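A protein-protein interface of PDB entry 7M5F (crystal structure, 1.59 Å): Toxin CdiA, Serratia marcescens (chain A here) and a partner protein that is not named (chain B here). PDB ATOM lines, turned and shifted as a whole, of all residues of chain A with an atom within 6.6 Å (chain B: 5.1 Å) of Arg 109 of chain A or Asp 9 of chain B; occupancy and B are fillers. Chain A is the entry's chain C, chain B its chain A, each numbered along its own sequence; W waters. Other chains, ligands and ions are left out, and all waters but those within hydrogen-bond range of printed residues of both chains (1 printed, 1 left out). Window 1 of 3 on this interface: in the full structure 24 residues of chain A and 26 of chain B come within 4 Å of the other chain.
The guanidinium group (NH1) of Arg 109 of chain A is in salt-bridge range of the side-chain carboxylate (OD2) of Asp 9 of chain B, 2.9 Å away. OE2 of Glu 71 of chain A lies close to O of Ala 8 of chain B. The side-chain carboxylate of Glu 71 of chain A lies close to the side-chain carboxylate of Asp 9 of chain B (3.1 Å). The side-chain carboxylate (OD2) of Asp 9 of chain B is in hydrogen-bond range of a ring nitrogen (NE2) of His 72 of chain A (2.8 Å). O of Tyr 10 of chain B is in hydrogen-bond range of NH2 of Arg 109 of chain A, at 3.0 Å. NH1 of Arg 109 of chain A sits close to SG of Cys 12 of chain B (3.6 Å). O of Glu 71 of chain A lies close to SD of Met 7 of chain B (3.4 Å). The side-chain amide nitrogen of Gln 103 of chain A lies within hydrogen-bond range of the side-chain sulfur of Cys 12 of chain B. OD1 of Asp 9 of chain B lies within hydrogen-bond range of NE2 of His 67 of chain A, at 2.8 Å. N of Arg 109 of chain A lies within hydrogen-bond range of O of His 11 of chain B (2.9 Å).
The backbone carbonyl oxygen of Tyr 10 of chain B lies within hydrogen-bond range of the side-chain sulfur of Cys 12 of chain B (3.4 Å). NH1 of Arg 109 of chain A is in hydrogen-bond range of OD1 of Asn 137 of chain A (3.0 Å). O of Gln 103 of chain A lies within hydrogen-bond range of N of Gly 108 of chain A. The backbone carbonyl oxygen (O) of Met 7 of chain B lies within hydrogen-bond range of the indole nitrogen (NE1) of Trp 16 of chain B, at 2.8 Å. N of Val 134 of chain A lies within hydrogen-bond range of O of Thr 126 of chain A (2.8 Å). The guanidinium group (NE) of Arg 109 of chain A is in hydrogen-bond range of the side-chain hydroxyl (OG1) of Thr 126 of chain A, 2.8 Å away.
His 67 of chain A touches Tyr 10 of chain B (NE2 to CE2, 3.8 Å). His 72 of chain A touches Met 7 of chain B. His 72 of chain A touches Trp 16 of chain B (CE1 to CZ3, 3.5 Å). C of Gln 103 of chain A touches O of His 11 of chain B (3.9 Å). Gly 104 of chain A touches His 11 of chain B (N to O, 3.8 Å). His 11 of chain B touches Gly 108 of chain A (O to CA, 3.4 Å). O of Tyr 10 of chain B touches OG1 of Thr 126 of chain A, at 3.5 Å. Thr 126 of chain A touches His 11 of chain B. Tyr 10 of chain B touches Val 134 of chain A. Asn 137 of chain A touches Trp 16 of chain B.
Printed residues of chain B within 4 Å of His 67 of chain A: Asp 9 (2.8 Å), Tyr 10 (3.8 Å) and Tyr 48 (3.0 Å). Ala 107 of chain A touches none of the printed residues of chain B. Arg 109 of chain A touches four residues of chain B. Tyr 112 of chain A touches none of the printed residues of chain B. Asp 9 of chain B touches just these residues of chain A: His 67, Glu 71, His 72 and Arg 109. Printed residues of chain A within 4 Å of His 11 of chain B: Gln 103, Gly 104, Gly 108, Arg 109 and Thr 126. The nearest residue of chain B that does not touch Arg 109 of chain A is Trp 16 of chain B (4.7 Å). The nearest residue of chain A that does not touch Asp 9 of chain B is Ala 136 of chain A (4.6 Å).
Hydrophobic or aromatic side chains of chain B that line the printed part of chain A: Met 7, Tyr 10, His 11, Trp 16 and Tyr 48. Along chain A the printed residues that touch a printed residue of chain B span positions 67 to 137. Among the printed residues, 21 pairs touch across the chains. Among the printed residues, Asp or Glu carboxylates within 4 Å of a Lys or Arg side-chain nitrogen of the other chain: Arg 109 of chain A with Asp 9 of chain B.
Water W1 lies within hydrogen-bond range of the side-chain carboxylate (OD2) of Asp 9 of chain B, the backbone NH (N) of Ala 136 of chain A and a ring nitrogen (NE2) of His 67 of chain A.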
ATOM      1  N   HIS A  67      31.278 -20.952  34.412  1.00  0.00           N
ATOM      2  CA  HIS A  67      30.282 -21.813  33.776  1.00  0.00           C
ATOM      3  C   HIS A  67      30.939 -22.889  32.918  1.00  0.00           C
ATOM      4  O   HIS A  67      30.509 -24.052  32.939  1.00  0.00           O
ATOM      5  CB  HIS A  67      29.352 -20.933  32.939  1.00  0.00           C
ATOM      6  CG  HIS A  67      28.334 -21.689  32.147  1.00  0.00           C
ATOM      7  ND1 HIS A  67      27.164 -22.154  32.697  1.00  0.00           N
ATOM      8  CD2 HIS A  67      28.315 -22.063  30.852  1.00  0.00           C
ATOM      9  CE1 HIS A  67      26.450 -22.773  31.764  1.00  0.00           C
ATOM     10  NE2 HIS A  67      27.128 -22.729  30.635  1.00  0.00           N
ATOM     11  N   ILE A  68      31.957 -22.517  32.147  1.00  0.00           N
ATOM     12  CA  ILE A  68      32.704 -23.489  31.350  1.00  0.00           C
ATOM     13  C   ILE A  68      33.327 -24.547  32.252  1.00  0.00           C
ATOM     14  O   ILE A  68      33.244 -25.752  31.973  1.00  0.00           O
ATOM     15  CB  ILE A  68      33.784 -22.777  30.511  1.00  0.00           C
ATOM     16  CG1 ILE A  68      33.147 -21.781  29.539  1.00  0.00           C
ATOM     17  CG2 ILE A  68      34.635 -23.801  29.780  1.00  0.00           C
ATOM     18  CD1 ILE A  68      34.142 -20.842  28.887  1.00  0.00           C
ATOM     19  N   GLU A  71      30.720 -26.856  34.208  1.00  0.00           N
ATOM     20  CA  GLU A  71      29.985 -27.738  33.307  1.00  0.00           C
ATOM     21  C   GLU A  71      30.900 -28.736  32.612  1.00  0.00           C
ATOM     22  O   GLU A  71      30.590 -29.924  32.566  1.00  0.00           O
ATOM     23  CB  GLU A  71      29.206 -26.970  32.241  1.00  0.00           C
ATOM     24  CG  GLU A  71      27.933 -26.366  32.769  1.00  0.00           C
ATOM     25  CD  GLU A  71      26.766 -26.404  31.806  1.00  0.00           C
ATOM     26  OE1 GLU A  71      26.967 -26.747  30.620  1.00  0.00           O
ATOM     27  OE2 GLU A  71      25.616 -26.118  32.240  1.00  0.00           O
ATOM     28  N   HIS A  72      32.025 -28.273  32.066  1.00  0.00           N
ATOM     29  CA  HIS A  72      32.811 -29.079  31.137  1.00  0.00           C
ATOM     30  C   HIS A  72      34.276 -29.202  31.520  1.00  0.00           C
ATOM     31  O   HIS A  72      35.089 -29.685  30.706  1.00  0.00           O
ATOM     32  CB  HIS A  72      32.731 -28.511  29.710  1.00  0.00           C
ATOM     33  CG  HIS A  72      31.349 -28.440  29.136  1.00  0.00           C
ATOM     34  ND1 HIS A  72      30.688 -29.540  28.635  1.00  0.00           N
ATOM     35  CD2 HIS A  72      30.518 -27.390  28.948  1.00  0.00           C
ATOM     36  CE1 HIS A  72      29.502 -29.171  28.188  1.00  0.00           C
ATOM     37  NE2 HIS A  72      29.384 -27.868  28.355  1.00  0.00           N
ATOM     38  N   GLY A 101      31.065 -26.567  12.060  1.00  0.00           N
ATOM     39  CA  GLY A 101      29.741 -27.120  12.275  1.00  0.00           C
ATOM     40  C   GLY A 101      29.080 -26.388  13.423  1.00  0.00           C
ATOM     41  O   GLY A 101      29.615 -25.407  13.938  1.00  0.00           O
ATOM     42  N   TYR A 102      27.910 -26.901  13.821  1.00  0.00           N
ATOM     43  CA  TYR A 102      27.084 -26.290  14.853  1.00  0.00           C
ATOM     44  C   TYR A 102      26.474 -27.376  15.718  1.00  0.00           C
ATOM     45  O   TYR A 102      26.066 -28.434  15.213  1.00  0.00           O
ATOM     46  CB  TYR A 102      25.965 -25.447  14.239  1.00  0.00           C
ATOM     47  CG  TYR A 102      26.487 -24.321  13.389  1.00  0.00           C
ATOM     48  CD1 TYR A 102      26.788 -24.523  12.056  1.00  0.00           C
ATOM     49  CD2 TYR A 102      26.739 -23.085  13.940  1.00  0.00           C
ATOM     50  CE1 TYR A 102      27.301 -23.499  11.284  1.00  0.00           C
ATOM     51  CE2 TYR A 102      27.245 -22.049  13.165  1.00  0.00           C
ATOM     52  CZ  TYR A 102      27.526 -22.277  11.838  1.00  0.00           C
ATOM     53  OH  TYR A 102      28.043 -21.260  11.054  1.00  0.00           O
ATOM     54  N   GLN A 103      26.415 -27.115  17.019  1.00  0.00           N
ATOM     55  CA  GLN A 103      25.779 -28.017  17.965  1.00  0.00           C
ATOM     56  C   GLN A 103      24.282 -27.727  18.023  1.00  0.00           C
ATOM     57  O   GLN A 103      23.756 -26.908  17.274  1.00  0.00           O
ATOM     58  CB  GLN A 103      26.449 -27.896  19.325  1.00  0.00           C
ATOM     59  CG  GLN A 103      27.894 -28.381  19.253  1.00  0.00           C
ATOM     60  CD  GLN A 103      28.599 -28.543  20.585  1.00  0.00           C
ATOM     61  OE1 GLN A 103      29.580 -29.277  20.677  1.00  0.00           O
ATOM     62  NE2 GLN A 103      28.118 -27.863  21.624  1.00  0.00           N
ATOM     63  N   GLY A 104      23.579 -28.427  18.908  1.00  0.00           N
ATOM     64  CA  GLY A 104      22.133 -28.361  18.843  1.00  0.00           C
ATOM     65  C   GLY A 104      21.642 -29.014  17.559  1.00  0.00           C
ATOM     66  O   GLY A 104      22.277 -29.920  17.008  1.00  0.00           O
ATOM     67  N   ALA A 107      22.039 -25.585  14.213  1.00  0.00           N
ATOM     68  CA  ALA A 107      22.084 -24.128  14.172  1.00  0.00           C
ATOM     69  C   ALA A 107      22.379 -23.555  15.556  1.00  0.00           C
ATOM     70  O   ALA A 107      22.072 -22.385  15.815  1.00  0.00           O
ATOM     71  CB  ALA A 107      20.765 -23.562  13.647  1.00  0.00           C
ATOM     72  N   GLY A 108      22.948 -24.362  16.446  1.00  0.00           N
ATOM     73  CA  GLY A 108      23.278 -23.925  17.782  1.00  0.00           C
ATOM     74  C   GLY A 108      24.708 -23.450  17.898  1.00  0.00           C
ATOM     75  O   GLY A 108      25.217 -22.741  17.028  1.00  0.00           O
ATOM     76  N   ARG A 109      25.361 -23.871  18.966  1.00  0.00           N
ATOM     77  CA  ARG A 109      26.684 -23.359  19.297  1.00  0.00           C
ATOM     78  C   ARG A 109      27.686 -23.690  18.194  1.00  0.00           C
ATOM     79  O   ARG A 109      27.852 -24.865  17.852  1.00  0.00           O
ATOM     80  CB  ARG A 109      27.123 -23.976  20.605  1.00  0.00           C
ATOM     81  CG  ARG A 109      28.509 -23.539  21.048  1.00  0.00           C
ATOM     82  CD  ARG A 109      28.842 -24.111  22.425  1.00  0.00           C
ATOM     83  NE  ARG A 109      27.997 -23.546  23.465  1.00  0.00           N
ATOM     84  CZ  ARG A 109      28.009 -23.905  24.734  1.00  0.00           C
ATOM     85  NH1 ARG A 109      28.793 -24.887  25.153  1.00  0.00           N
ATOM     86  NH2 ARG A 109      27.190 -23.314  25.570  1.00  0.00           N
ATOM     87  N   PRO A 110      28.393 -22.701  17.657  1.00  0.00           N
ATOM     88  CA  PRO A 110      29.400 -22.989  16.624  1.00  0.00           C
ATOM     89  C   PRO A 110      30.563 -23.807  17.151  1.00  0.00           C
ATOM     90  O   PRO A 110      31.029 -23.631  18.275  1.00  0.00           O
ATOM     91  CB  PRO A 110      29.871 -21.593  16.178  1.00  0.00           C
ATOM     92  CG  PRO A 110      28.806 -20.664  16.649  1.00  0.00           C
ATOM     93  CD  PRO A 110      28.220 -21.249  17.864  1.00  0.00           C
ATOM     94  N   ILE A 111      31.050 -24.715  16.292  1.00  0.00           N
ATOM     95  CA  ILE A 111      32.183 -25.593  16.565  1.00  0.00           C
ATOM     96  C   ILE A 111      33.392 -25.029  15.827  1.00  0.00           C
ATOM     97  O   ILE A 111      33.363 -24.945  14.599  1.00  0.00           O
ATOM     98  CB  ILE A 111      31.894 -27.024  16.092  1.00  0.00           C
ATOM     99  CG1 ILE A 111      30.617 -27.547  16.742  1.00  0.00           C
ATOM    100  CG2 ILE A 111      33.071 -27.942  16.397  1.00  0.00           C
ATOM    101  CD1 ILE A 111      30.043 -28.769  16.054  1.00  0.00           C
ATOM    102  N   TYR A 112      34.468 -24.731  16.564  1.00  0.00           N
ATOM    103  CA  TYR A 112      35.690 -24.169  16.004  1.00  0.00           C
ATOM    104  C   TYR A 112      36.799 -25.219  15.964  1.00  0.00           C
ATOM    105  O   TYR A 112      37.150 -25.806  16.996  1.00  0.00           O
ATOM    106  CB  TYR A 112      36.165 -22.964  16.819  1.00  0.00           C
ATOM    107  CG  TYR A 112      35.186 -21.811  16.806  1.00  0.00           C
ATOM    108  CD1 TYR A 112      34.165 -21.750  17.727  1.00  0.00           C
ATOM    109  CD2 TYR A 112      35.270 -20.815  15.850  1.00  0.00           C
ATOM    110  CE1 TYR A 112      33.254 -20.711  17.702  1.00  0.00           C
ATOM    111  CE2 TYR A 112      34.369 -19.778  15.822  1.00  0.00           C
ATOM    112  CZ  TYR A 112      33.357 -19.734  16.749  1.00  0.00           C
ATOM    113  OH  TYR A 112      32.450 -18.691  16.710  1.00  0.00           O
ATOM    114  N   ILE A 123      36.448 -27.169  19.415  1.00  0.00           N
ATOM    115  CA  ILE A 123      35.943 -26.526  20.607  1.00  0.00           C
ATOM    116  C   ILE A 123      34.750 -25.676  20.194  1.00  0.00           C
ATOM    117  O   ILE A 123      34.878 -24.810  19.323  1.00  0.00           O
ATOM    118  CB  ILE A 123      37.017 -25.668  21.306  1.00  0.00           C
ATOM    119  CG1 ILE A 123      38.196 -26.524  21.715  1.00  0.00           C
ATOM    120  CG2 ILE A 123      36.417 -24.976  22.513  1.00  0.00           C
ATOM    121  CD1 ILE A 123      39.249 -25.763  22.486  1.00  0.00           C
ATOM    122  N   ALA A 124      33.586 -25.963  20.769  1.00  0.00           N
ATOM    123  CA  ALA A 124      32.374 -25.183  20.508  1.00  0.00           C
ATOM    124  C   ALA A 124      32.295 -24.045  21.517  1.00  0.00           C
ATOM    125  O   ALA A 124      32.585 -24.237  22.702  1.00  0.00           O
ATOM    126  CB  ALA A 124      31.143 -26.089  20.584  1.00  0.00           C
ATOM    127  N   VAL A 125      31.904 -22.848  21.051  1.00  0.00           N
ATOM    128  CA  VAL A 125      31.905 -21.660  21.895  1.00  0.00           C
ATOM    129  C   VAL A 125      30.680 -20.810  21.570  1.00  0.00           C
ATOM    130  O   VAL A 125      30.471 -20.440  20.416  1.00  0.00           O
ATOM    131  CB  VAL A 125      33.183 -20.810  21.725  1.00  0.00           C
ATOM    132  CG1 VAL A 125      33.212 -19.680  22.762  1.00  0.00           C
ATOM    133  CG2 VAL A 125      34.451 -21.651  21.848  1.00  0.00           C
ATOM    134  N   THR A 126      29.896 -20.475  22.598  1.00  0.00           N
ATOM    135  CA  THR A 126      28.805 -19.513  22.507  1.00  0.00           C
ATOM    136  C   THR A 126      29.308 -18.150  22.991  1.00  0.00           C
ATOM    137  O   THR A 126      29.894 -18.063  24.070  1.00  0.00           O
ATOM    138  CB  THR A 126      27.617 -19.933  23.370  1.00  0.00           C
ATOM    139  OG1 THR A 126      26.948 -21.060  22.784  1.00  0.00           O
ATOM    140  CG2 THR A 126      26.587 -18.829  23.508  1.00  0.00           C
ATOM    141  N   VAL A 127      29.027 -17.112  22.203  1.00  0.00           N
ATOM    142  CA  VAL A 127      29.443 -15.734  22.471  1.00  0.00           C
ATOM    143  C   VAL A 127      28.215 -14.842  22.367  1.00  0.00           C
ATOM    144  O   VAL A 127      27.393 -15.003  21.455  1.00  0.00           O
ATOM    145  CB  VAL A 127      30.526 -15.272  21.482  1.00  0.00           C
ATOM    146  CG1 VAL A 127      30.949 -13.843  21.752  1.00  0.00           C
ATOM    147  CG2 VAL A 127      31.726 -16.161  21.566  1.00  0.00           C
ATOM    148  N   VAL A 134      30.203 -16.982  26.640  1.00  0.00           N
ATOM    149  CA  VAL A 134      29.157 -17.491  27.530  1.00  0.00           C
ATOM    150  C   VAL A 134      29.482 -18.894  28.018  1.00  0.00           C
ATOM    151  O   VAL A 134      29.426 -19.170  29.215  1.00  0.00           O
ATOM    152  CB  VAL A 134      27.796 -17.480  26.821  1.00  0.00           C
ATOM    153  CG1 VAL A 134      26.707 -17.974  27.749  1.00  0.00           C
ATOM    154  CG2 VAL A 134      27.418 -16.118  26.295  1.00  0.00           C
ATOM    155  N   GLY A 135      29.793 -19.792  27.085  1.00  0.00           N
ATOM    156  CA  GLY A 135      30.052 -21.182  27.421  1.00  0.00           C
ATOM    157  C   GLY A 135      30.829 -21.826  26.296  1.00  0.00           C
ATOM    158  O   GLY A 135      30.936 -21.288  25.195  1.00  0.00           O
ATOM    159  N   ALA A 136      31.381 -22.994  26.594  1.00  0.00           N
ATOM    160  CA  ALA A 136      32.282 -23.652  25.653  1.00  0.00           C
ATOM    161  C   ALA A 136      32.405 -25.113  26.038  1.00  0.00           C
ATOM    162  O   ALA A 136      32.276 -25.471  27.209  1.00  0.00           O
ATOM    163  CB  ALA A 136      33.677 -23.019  25.640  1.00  0.00           C
ATOM    164  N   ASN A 137      32.728 -25.944  25.048  1.00  0.00           N
ATOM    165  CA  ASN A 137      32.942 -27.352  25.311  1.00  0.00           C
ATOM    166  C   ASN A 137      33.845 -27.944  24.239  1.00  0.00           C
ATOM    167  O   ASN A 137      33.890 -27.465  23.105  1.00  0.00           O
ATOM    168  CB  ASN A 137      31.621 -28.150  25.369  1.00  0.00           C
ATOM    169  CG  ASN A 137      30.853 -28.136  24.066  1.00  0.00           C
ATOM    170  OD1 ASN A 137      30.009 -27.262  23.842  1.00  0.00           O
ATOM    171  ND2 ASN A 137      31.140 -29.094  23.191  1.00  0.00           N
ATOM    172  N   MET B   7      22.708 -32.567  31.105  1.00  0.00           N
ATOM    173  CA  MET B   7      23.180 -31.262  31.516  1.00  0.00           C
ATOM    174  C   MET B   7      22.790 -30.245  30.479  1.00  0.00           C
ATOM    175  O   MET B   7      23.116 -30.392  29.301  1.00  0.00           O
ATOM    176  CB  MET B   7      24.693 -31.288  31.688  1.00  0.00           C
ATOM    177  CG  MET B   7      25.267 -29.977  32.138  1.00  0.00           C
ATOM    178  SD  MET B   7      27.160 -30.012  32.494  1.00  0.00           S
ATOM    179  CE  MET B   7      27.751 -30.202  30.687  1.00  0.00           C
ATOM    180  N   ALA B   8      22.095 -29.200  30.897  1.00  0.00           N
ATOM    181  CA  ALA B   8      21.739 -28.147  29.965  1.00  0.00           C
ATOM    182  C   ALA B   8      22.903 -27.185  29.781  1.00  0.00           C
ATOM    183  O   ALA B   8      23.599 -26.840  30.732  1.00  0.00           O
ATOM    184  CB  ALA B   8      20.504 -27.402  30.461  1.00  0.00           C
ATOM    185  N   ASP B   9      23.132 -26.784  28.533  1.00  0.00           N
ATOM    186  CA  ASP B   9      24.077 -25.742  28.166  1.00  0.00           C
ATOM    187  C   ASP B   9      23.487 -24.978  26.990  1.00  0.00           C
ATOM    188  O   ASP B   9      22.783 -25.541  26.154  1.00  0.00           O
ATOM    189  CB  ASP B   9      25.476 -26.316  27.837  1.00  0.00           C
ATOM    190  CG  ASP B   9      26.591 -25.299  28.034  1.00  0.00           C
ATOM    191  OD1 ASP B   9      26.299 -24.136  28.398  1.00  0.00           O
ATOM    192  OD2 ASP B   9      27.762 -25.685  27.787  1.00  0.00           O
ATOM    193  N   TYR B  10      23.800 -23.695  26.921  1.00  0.00           N
ATOM    194  CA  TYR B  10      23.168 -22.823  25.944  1.00  0.00           C
ATOM    195  C   TYR B  10      23.452 -23.262  24.513  1.00  0.00           C
ATOM    196  O   TYR B  10      24.604 -23.375  24.102  1.00  0.00           O
ATOM    197  CB  TYR B  10      23.661 -21.405  26.141  1.00  0.00           C
ATOM    198  CG  TYR B  10      23.504 -20.877  27.540  1.00  0.00           C
ATOM    199  CD1 TYR B  10      22.258 -20.549  28.042  1.00  0.00           C
ATOM    200  CD2 TYR B  10      24.603 -20.689  28.356  1.00  0.00           C
ATOM    201  CE1 TYR B  10      22.109 -20.031  29.301  1.00  0.00           C
ATOM    202  CE2 TYR B  10      24.464 -20.176  29.633  1.00  0.00           C
ATOM    203  CZ  TYR B  10      23.210 -19.846  30.102  1.00  0.00           C
ATOM    204  OH  TYR B  10      23.024 -19.315  31.351  1.00  0.00           O
ATOM    205  N   HIS B  11      22.382 -23.393  23.726  1.00  0.00           N
ATOM    206  CA  HIS B  11      22.460 -23.682  22.291  1.00  0.00           C
ATOM    207  C   HIS B  11      23.092 -25.033  22.008  1.00  0.00           C
ATOM    208  O   HIS B  11      23.682 -25.225  20.945  1.00  0.00           O
ATOM    209  CB  HIS B  11      23.184 -22.574  21.548  1.00  0.00           C
ATOM    210  CG  HIS B  11      22.552 -21.231  21.725  1.00  0.00           C
ATOM    211  ND1 HIS B  11      21.202 -21.024  21.557  1.00  0.00           N
ATOM    212  CD2 HIS B  11      23.081 -20.035  22.074  1.00  0.00           C
ATOM    213  CE1 HIS B  11      20.927 -19.746  21.782  1.00  0.00           C
ATOM    214  NE2 HIS B  11      22.049 -19.125  22.091  1.00  0.00           N
ATOM    215  N   CYS B  12      22.897 -25.960  22.940  1.00  0.00           N
ATOM    216  CA  CYS B  12      23.341 -27.335  22.839  1.00  0.00           C
ATOM    217  C   CYS B  12      22.200 -28.280  23.168  1.00  0.00           C
ATOM    218  O   CYS B  12      21.293 -27.946  23.932  1.00  0.00           O
ATOM    219  CB  CYS B  12      24.457 -27.629  23.821  1.00  0.00           C
ATOM    220  SG  CYS B  12      25.906 -26.534  23.698  1.00  0.00           S
ATOM    221  N   TRP B  16      25.343 -35.410  26.860  1.00  0.00           N
ATOM    222  CA  TRP B  16      26.774 -35.283  26.602  1.00  0.00           C
ATOM    223  C   TRP B  16      27.505 -36.607  26.733  1.00  0.00           C
ATOM    224  O   TRP B  16      27.228 -37.392  27.640  1.00  0.00           O
ATOM    225  CB  TRP B  16      27.421 -34.265  27.579  1.00  0.00           C
ATOM    226  CG  TRP B  16      26.787 -32.926  27.497  1.00  0.00           C
ATOM    227  CD1 TRP B  16      25.658 -32.526  28.142  1.00  0.00           C
ATOM    228  CD2 TRP B  16      27.200 -31.826  26.688  1.00  0.00           C
ATOM    229  NE1 TRP B  16      25.349 -31.255  27.789  1.00  0.00           N
ATOM    230  CE2 TRP B  16      26.277 -30.792  26.896  1.00  0.00           C
ATOM    231  CE3 TRP B  16      28.264 -31.625  25.799  1.00  0.00           C
ATOM    232  CZ2 TRP B  16      26.386 -29.544  26.264  1.00  0.00           C
ATOM    233  CZ3 TRP B  16      28.369 -30.390  25.155  1.00  0.00           C
ATOM    234  CH2 TRP B  16      27.432 -29.367  25.400  1.00  0.00           C
ATOM    235  N   TYR B  48      16.264 -23.704  29.546  1.00  0.00           N
ATOM    236  CA  TYR B  48      17.565 -23.167  29.899  1.00  0.00           C
ATOM    237  C   TYR B  48      18.004 -22.120  28.889  1.00  0.00           C
ATOM    238  O   TYR B  48      18.525 -21.074  29.267  1.00  0.00           O
ATOM    239  CB  TYR B  48      18.597 -24.294  30.004  1.00  0.00           C
ATOM    240  CG  TYR B  48      19.899 -23.843  30.641  1.00  0.00           C
ATOM    241  CD1 TYR B  48      19.975 -23.580  31.991  1.00  0.00           C
ATOM    242  CD2 TYR B  48      21.062 -23.705  29.879  1.00  0.00           C
ATOM    243  CE1 TYR B  48      21.165 -23.171  32.565  1.00  0.00           C
ATOM    244  CE2 TYR B  48      22.230 -23.300  30.439  1.00  0.00           C
ATOM    245  CZ  TYR B  48      22.284 -23.055  31.792  1.00  0.00           C
ATOM    246  OH  TYR B  48      23.480 -22.651  32.335  1.00  0.00           O
ATOM    247  N   ASP B  49      17.823 -22.393  27.598  1.00  0.00           N
ATOM    248  CA  ASP B  49      18.188 -21.402  26.596  1.00  0.00           C
ATOM    249  C   ASP B  49      17.498 -20.073  26.866  1.00  0.00           C
ATOM    250  O   ASP B  49      18.051 -19.009  26.563  1.00  0.00           O
ATOM    251  CB  ASP B  49      17.825 -21.899  25.194  1.00  0.00           C
ATOM    252  CG  ASP B  49      18.767 -22.962  24.671  1.00  0.00           C
ATOM    253  OD1 ASP B  49      19.892 -23.104  25.170  1.00  0.00           O
ATOM    254  OD2 ASP B  49      18.354 -23.678  23.722  1.00  0.00           O
HETATM  255  O   HOH W   1      29.826 -24.089  28.983  1.00  0.00           O
